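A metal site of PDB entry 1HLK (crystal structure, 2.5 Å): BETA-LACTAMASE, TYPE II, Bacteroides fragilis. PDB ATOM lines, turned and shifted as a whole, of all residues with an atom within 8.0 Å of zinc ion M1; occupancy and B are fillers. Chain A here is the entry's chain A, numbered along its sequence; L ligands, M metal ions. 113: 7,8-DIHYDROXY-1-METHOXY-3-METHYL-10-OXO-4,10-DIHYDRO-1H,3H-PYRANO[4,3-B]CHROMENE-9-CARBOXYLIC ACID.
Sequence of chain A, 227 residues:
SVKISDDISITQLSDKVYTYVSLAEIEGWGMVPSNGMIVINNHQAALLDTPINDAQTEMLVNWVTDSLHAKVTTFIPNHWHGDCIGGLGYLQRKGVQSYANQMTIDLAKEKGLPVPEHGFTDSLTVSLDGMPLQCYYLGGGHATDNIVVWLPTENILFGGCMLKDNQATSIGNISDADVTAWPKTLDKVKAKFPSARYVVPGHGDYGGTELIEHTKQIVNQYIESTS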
ATOM      1  N   ASP A  49     -29.718  -9.487  10.365  1.00  0.00           N
ATOM      2  CA  ASP A  49     -30.349 -10.590   9.660  1.00  0.00           C
ATOM      3  C   ASP A  49     -31.286 -11.296  10.626  1.00  0.00           C
ATOM      4  O   ASP A  49     -31.039 -11.334  11.833  1.00  0.00           O
ATOM      5  CB  ASP A  49     -29.308 -11.590   9.152  1.00  0.00           C
ATOM      6  CG  ASP A  49     -28.604 -11.113   7.910  1.00  0.00           C
ATOM      7  OD1 ASP A  49     -28.454  -9.894   7.759  1.00  0.00           O
ATOM      8  OD2 ASP A  49     -28.188 -11.968   7.095  1.00  0.00           O
ATOM      9  N   ASN A  78     -28.770  -7.866   5.659  1.00  0.00           N
ATOM     10  CA  ASN A  78     -27.621  -7.881   4.755  1.00  0.00           C
ATOM     11  C   ASN A  78     -28.041  -7.534   3.325  1.00  0.00           C
ATOM     12  O   ASN A  78     -27.309  -6.822   2.610  1.00  0.00           O
ATOM     13  CB  ASN A  78     -26.920  -9.238   4.792  1.00  0.00           C
ATOM     14  CG  ASN A  78     -25.634  -9.255   3.978  1.00  0.00           C
ATOM     15  OD1 ASN A  78     -25.644  -9.458   2.770  1.00  0.00           O
ATOM     16  ND2 ASN A  78     -24.527  -9.007   4.652  1.00  0.00           N
ATOM     17  N   HIS A  79     -29.192  -8.060   2.920  1.00  0.00           N
ATOM     18  CA  HIS A  79     -29.788  -7.792   1.612  1.00  0.00           C
ATOM     19  C   HIS A  79     -31.237  -8.322   1.589  1.00  0.00           C
ATOM     20  O   HIS A  79     -31.710  -8.876   2.584  1.00  0.00           O
ATOM     21  CB  HIS A  79     -28.945  -8.364   0.451  1.00  0.00           C
ATOM     22  CG  HIS A  79     -28.670  -9.824   0.530  1.00  0.00           C
ATOM     23  ND1 HIS A  79     -27.899 -10.388   1.528  1.00  0.00           N
ATOM     24  CD2 HIS A  79     -29.092 -10.859  -0.233  1.00  0.00           C
ATOM     25  CE1 HIS A  79     -27.861 -11.707   1.368  1.00  0.00           C
ATOM     26  NE2 HIS A  79     -28.578 -12.011   0.304  1.00  0.00           N
ATOM     27  N   TRP A  80     -31.933  -8.137   0.475  1.00  0.00           N
ATOM     28  CA  TRP A  80     -33.332  -8.527   0.364  1.00  0.00           C
ATOM     29  C   TRP A  80     -33.789  -9.980   0.417  1.00  0.00           C
ATOM     30  O   TRP A  80     -35.003 -10.214   0.428  1.00  0.00           O
ATOM     31  CB  TRP A  80     -33.955  -7.925  -0.899  1.00  0.00           C
ATOM     32  CG  TRP A  80     -33.400  -8.482  -2.176  1.00  0.00           C
ATOM     33  CD1 TRP A  80     -32.210  -8.165  -2.753  1.00  0.00           C
ATOM     34  CD2 TRP A  80     -34.013  -9.452  -3.027  1.00  0.00           C
ATOM     35  NE1 TRP A  80     -32.041  -8.881  -3.915  1.00  0.00           N
ATOM     36  CE2 TRP A  80     -33.139  -9.678  -4.112  1.00  0.00           C
ATOM     37  CE3 TRP A  80     -35.227 -10.160  -2.979  1.00  0.00           C
ATOM     38  CZ2 TRP A  80     -33.434 -10.581  -5.145  1.00  0.00           C
ATOM     39  CZ3 TRP A  80     -35.523 -11.066  -4.003  1.00  0.00           C
ATOM     40  CH2 TRP A  80     -34.627 -11.261  -5.076  1.00  0.00           C
ATOM     41  N   HIS A  81     -32.874 -10.944   0.472  1.00  0.00           N
ATOM     42  CA  HIS A  81     -33.277 -12.350   0.505  1.00  0.00           C
ATOM     43  C   HIS A  81     -33.929 -12.826   1.784  1.00  0.00           C
ATOM     44  O   HIS A  81     -33.841 -12.180   2.831  1.00  0.00           O
ATOM     45  CB  HIS A  81     -32.114 -13.273   0.140  1.00  0.00           C
ATOM     46  CG  HIS A  81     -31.805 -13.293  -1.321  1.00  0.00           C
ATOM     47  ND1 HIS A  81     -30.621 -13.806  -1.823  1.00  0.00           N
ATOM     48  CD2 HIS A  81     -32.517 -12.883  -2.390  1.00  0.00           C
ATOM     49  CE1 HIS A  81     -30.633 -13.710  -3.142  1.00  0.00           C
ATOM     50  NE2 HIS A  81     -31.768 -13.148  -3.513  1.00  0.00           N
ATOM     51  N   GLY A  82     -34.605 -13.973   1.671  1.00  0.00           N
ATOM     52  CA  GLY A  82     -35.312 -14.567   2.793  1.00  0.00           C
ATOM     53  C   GLY A  82     -34.490 -14.743   4.051  1.00  0.00           C
ATOM     54  O   GLY A  82     -34.970 -14.505   5.157  1.00  0.00           O
ATOM     55  N   ASP A  83     -33.241 -15.161   3.880  1.00  0.00           N
ATOM     56  CA  ASP A  83     -32.370 -15.376   5.017  1.00  0.00           C
ATOM     57  C   ASP A  83     -31.763 -14.095   5.603  1.00  0.00           C
ATOM     58  O   ASP A  83     -30.734 -14.129   6.288  1.00  0.00           O
ATOM     59  CB  ASP A  83     -31.284 -16.395   4.645  1.00  0.00           C
ATOM     60  CG  ASP A  83     -30.595 -16.096   3.327  1.00  0.00           C
ATOM     61  OD1 ASP A  83     -31.308 -15.947   2.306  1.00  0.00           O
ATOM     62  OD2 ASP A  83     -29.345 -16.023   3.304  1.00  0.00           O
ATOM     63  N   CYS A  84     -32.416 -12.967   5.346  1.00  0.00           N
ATOM     64  CA  CYS A  84     -31.966 -11.682   5.873  1.00  0.00           C
ATOM     65  C   CYS A  84     -33.142 -10.917   6.504  1.00  0.00           C
ATOM     66  O   CYS A  84     -33.047 -10.453   7.644  1.00  0.00           O
ATOM     67  CB  CYS A  84     -31.309 -10.857   4.772  1.00  0.00           C
ATOM     68  SG  CYS A  84     -29.925 -11.668   3.953  1.00  0.00           S
ATOM     69  N   HIS A 142     -22.744 -11.051  -4.006  1.00  0.00           N
ATOM     70  CA  HIS A 142     -23.715 -12.137  -3.948  1.00  0.00           C
ATOM     71  C   HIS A 142     -25.042 -11.597  -4.444  1.00  0.00           C
ATOM     72  O   HIS A 142     -25.800 -12.278  -5.121  1.00  0.00           O
ATOM     73  CB  HIS A 142     -23.896 -12.627  -2.519  1.00  0.00           C
ATOM     74  CG  HIS A 142     -25.154 -13.401  -2.319  1.00  0.00           C
ATOM     75  ND1 HIS A 142     -25.367 -14.636  -2.874  1.00  0.00           N
ATOM     76  CD2 HIS A 142     -26.315 -13.065  -1.699  1.00  0.00           C
ATOM     77  CE1 HIS A 142     -26.597 -15.030  -2.619  1.00  0.00           C
ATOM     78  NE2 HIS A 142     -27.198 -14.099  -1.898  1.00  0.00           N
ATOM     79  N   ALA A 143     -25.317 -10.353  -4.062  1.00  0.00           N
ATOM     80  CA  ALA A 143     -26.528  -9.654  -4.422  1.00  0.00           C
ATOM     81  C   ALA A 143     -26.100  -8.243  -4.808  1.00  0.00           C
ATOM     82  O   ALA A 143     -25.003  -7.824  -4.493  1.00  0.00           O
ATOM     83  CB  ALA A 143     -27.487  -9.639  -3.233  1.00  0.00           C
ATOM     84  N   ASP A 145     -27.461  -5.455  -3.728  1.00  0.00           N
ATOM     85  CA  ASP A 145     -27.618  -4.576  -2.579  1.00  0.00           C
ATOM     86  C   ASP A 145     -26.826  -4.921  -1.323  1.00  0.00           C
ATOM     87  O   ASP A 145     -26.854  -4.151  -0.358  1.00  0.00           O
ATOM     88  CB  ASP A 145     -29.106  -4.466  -2.204  1.00  0.00           C
ATOM     89  CG  ASP A 145     -29.756  -5.825  -1.883  1.00  0.00           C
ATOM     90  OD1 ASP A 145     -30.521  -5.893  -0.894  1.00  0.00           O
ATOM     91  OD2 ASP A 145     -29.543  -6.813  -2.617  1.00  0.00           O
ATOM     92  N   ASN A 146     -26.149  -6.058  -1.318  1.00  0.00           N
ATOM     93  CA  ASN A 146     -25.398  -6.511  -0.141  1.00  0.00           C
ATOM     94  C   ASN A 146     -24.405  -5.527   0.519  1.00  0.00           C
ATOM     95  O   ASN A 146     -23.623  -4.854  -0.149  1.00  0.00           O
ATOM     96  CB  ASN A 146     -24.678  -7.833  -0.460  1.00  0.00           C
ATOM     97  CG  ASN A 146     -23.571  -7.694  -1.522  1.00  0.00           C
ATOM     98  OD1 ASN A 146     -22.995  -8.698  -1.942  1.00  0.00           O
ATOM     99  ND2 ASN A 146     -23.288  -6.461  -1.947  1.00  0.00           N
ATOM    100  N   GLY A 160     -21.911 -11.355   5.627  1.00  0.00           N
ATOM    101  CA  GLY A 160     -23.080 -11.835   4.907  1.00  0.00           C
ATOM    102  C   GLY A 160     -22.703 -12.888   3.880  1.00  0.00           C
ATOM    103  O   GLY A 160     -21.671 -13.556   3.985  1.00  0.00           O
ATOM    104  N   CYS A 161     -23.527 -13.033   2.861  1.00  0.00           N
ATOM    105  CA  CYS A 161     -23.306 -14.032   1.842  1.00  0.00           C
ATOM    106  C   CYS A 161     -22.304 -13.652   0.776  1.00  0.00           C
ATOM    107  O   CYS A 161     -22.029 -14.435  -0.140  1.00  0.00           O
ATOM    108  CB  CYS A 161     -24.659 -14.420   1.211  1.00  0.00           C
ATOM    109  SG  CYS A 161     -25.831 -15.056   2.452  1.00  0.00           S
ATOM    110  N   MET A 162     -21.741 -12.453   0.859  1.00  0.00           N
ATOM    111  CA  MET A 162     -20.730 -12.138  -0.151  1.00  0.00           C
ATOM    112  C   MET A 162     -19.489 -12.922   0.240  1.00  0.00           C
ATOM    113  O   MET A 162     -18.610 -13.154  -0.573  1.00  0.00           O
ATOM    114  CB  MET A 162     -20.405 -10.628  -0.215  1.00  0.00           C
ATOM    115  CG  MET A 162     -19.403 -10.108   0.802  1.00  0.00           C
ATOM    116  SD  MET A 162     -18.877  -8.452   0.366  1.00  0.00           S
ATOM    117  CE  MET A 162     -20.453  -7.546   0.359  1.00  0.00           C
ATOM    118  N   ASN A 173     -25.705 -19.936  -4.782  1.00  0.00           N
ATOM    119  CA  ASN A 173     -26.846 -19.295  -5.446  1.00  0.00           C
ATOM    120  C   ASN A 173     -26.499 -17.942  -6.069  1.00  0.00           C
ATOM    121  O   ASN A 173     -26.568 -16.910  -5.409  1.00  0.00           O
ATOM    122  CB  ASN A 173     -27.983 -19.112  -4.438  1.00  0.00           C
ATOM    123  CG  ASN A 173     -29.189 -18.413  -5.039  1.00  0.00           C
ATOM    124  OD1 ASN A 173     -29.769 -18.883  -6.020  1.00  0.00           O
ATOM    125  ND2 ASN A 173     -29.574 -17.286  -4.454  1.00  0.00           N
ATOM    126  N   ASP A 176     -29.094 -13.657  -8.193  1.00  0.00           N
ATOM    127  CA  ASP A 176     -29.230 -12.210  -8.090  1.00  0.00           C
ATOM    128  C   ASP A 176     -27.840 -11.620  -7.951  1.00  0.00           C
ATOM    129  O   ASP A 176     -27.672 -10.440  -7.671  1.00  0.00           O
ATOM    130  CB  ASP A 176     -30.043 -11.855  -6.854  1.00  0.00           C
ATOM    131  CG  ASP A 176     -31.439 -12.409  -6.909  1.00  0.00           C
ATOM    132  OD1 ASP A 176     -32.238 -11.892  -7.704  1.00  0.00           O
ATOM    133  OD2 ASP A 176     -31.734 -13.371  -6.173  1.00  0.00           O
ATOM    134  N   HIS A 203     -23.249 -18.098   5.548  1.00  0.00           N
ATOM    135  CA  HIS A 203     -23.495 -19.530   5.665  1.00  0.00           C
ATOM    136  C   HIS A 203     -22.168 -20.210   5.962  1.00  0.00           C
ATOM    137  O   HIS A 203     -21.197 -19.973   5.259  1.00  0.00           O
ATOM    138  CB  HIS A 203     -24.057 -20.116   4.358  1.00  0.00           C
ATOM    139  CG  HIS A 203     -25.408 -19.571   3.986  1.00  0.00           C
ATOM    140  ND1 HIS A 203     -26.564 -19.920   4.653  1.00  0.00           N
ATOM    141  CD2 HIS A 203     -25.778 -18.681   3.041  1.00  0.00           C
ATOM    142  CE1 HIS A 203     -27.582 -19.257   4.138  1.00  0.00           C
ATOM    143  NE2 HIS A 203     -27.130 -18.502   3.159  1.00  0.00           N
HETATM  144  C1  113 L   1     -29.368 -20.158  -0.697  1.00  0.00           C
HETATM  145  C2  113 L   1     -29.013 -21.501  -0.572  1.00  0.00           C
HETATM  146  C3  113 L   1     -27.696 -21.832  -0.299  1.00  0.00           C
HETATM  147  C4  113 L   1     -26.708 -20.827  -0.211  1.00  0.00           C
HETATM  148  C5  113 L   1     -27.024 -19.528  -0.690  1.00  0.00           C
HETATM  149  C6  113 L   1     -28.379 -19.178  -0.847  1.00  0.00           C
HETATM  150  O8  113 L   1     -27.361 -23.159  -0.110  1.00  0.00           O
HETATM  151  C9  113 L   1     -26.066 -23.559   0.151  1.00  0.00           C
HETATM  152  C10 113 L   1     -25.075 -22.679   0.423  1.00  0.00           C
HETATM  153  C11 113 L   1     -25.411 -21.208   0.392  1.00  0.00           C
HETATM  154  C12 113 L   1     -25.853 -25.042   0.100  1.00  0.00           C
HETATM  155  C13 113 L   1     -24.381 -25.385  -0.168  1.00  0.00           C
HETATM  156  O14 113 L   1     -23.514 -24.592   0.650  1.00  0.00           O
HETATM  157  C15 113 L   1     -23.667 -23.168   0.744  1.00  0.00           C
HETATM  158  O16 113 L   1     -28.829 -17.901  -1.161  1.00  0.00           O
HETATM  159  O17 113 L   1     -30.676 -19.722  -0.664  1.00  0.00           O
HETATM  160  C18 113 L   1     -25.989 -18.531  -1.030  1.00  0.00           C
HETATM  161  O19 113 L   1     -25.765 -17.598  -0.081  1.00  0.00           O
HETATM  162  O20 113 L   1     -22.643 -22.471   0.040  1.00  0.00           O
HETATM  163  C22 113 L   1     -22.335 -22.777  -1.308  1.00  0.00           C
HETATM  164  C26 113 L   1     -24.045 -26.861   0.071  1.00  0.00           C
HETATM  165  O30 113 L   1     -25.381 -18.565  -2.069  1.00  0.00           O
HETATM  166  O31 113 L   1     -24.622 -20.421   0.873  1.00  0.00           O
HETATM  167 ZN    ZN M   1     -28.840 -14.096  -0.407  1.00  0.00          ZN
HETATM  168 ZN    ZN M   2     -27.259 -16.302   1.533  1.00  0.00          ZN
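Zinc ion M1 is bound by NE2 of His 142 (2.2 Å), NE2 of His 79 (2.2 Å) and ND1 of His 81 (2.3 Å).
Zinc ion M1 has three donor atoms within binding distance.
N of Asn 173 sits at hydrogen-bond distance from O30 of the ligand, at 3.1 Å.
An oxygen (O16) of the ligand lies within hydrogen-bond range of the side-chain amide nitrogen of Asn 173, at 3.4 Å.
The backbone NH (N) of His 142 is in hydrogen-bond range of the side-chain amide oxygen (OD1) of Asn 146, at 3.1 Å.
ND1 of His 79 sits close to SG of Cys 84, at 3.4 Å.
The side-chain amide oxygen (OD1) of Asn 78 lies within hydrogen-bond range of a ring nitrogen (ND1) of His 79 (2.7 Å).
A ring nitrogen (NE2) of His 81 sits at hydrogen-bond distance from the side-chain carboxylate (OD2) of Asp 176.
Three residues have an atom within 4 Å of zinc ion M1: His 79, His 81 and His 142.
The nearest printed residue that does not touch zinc ion M1 is Asp 83 (4.1 Å).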
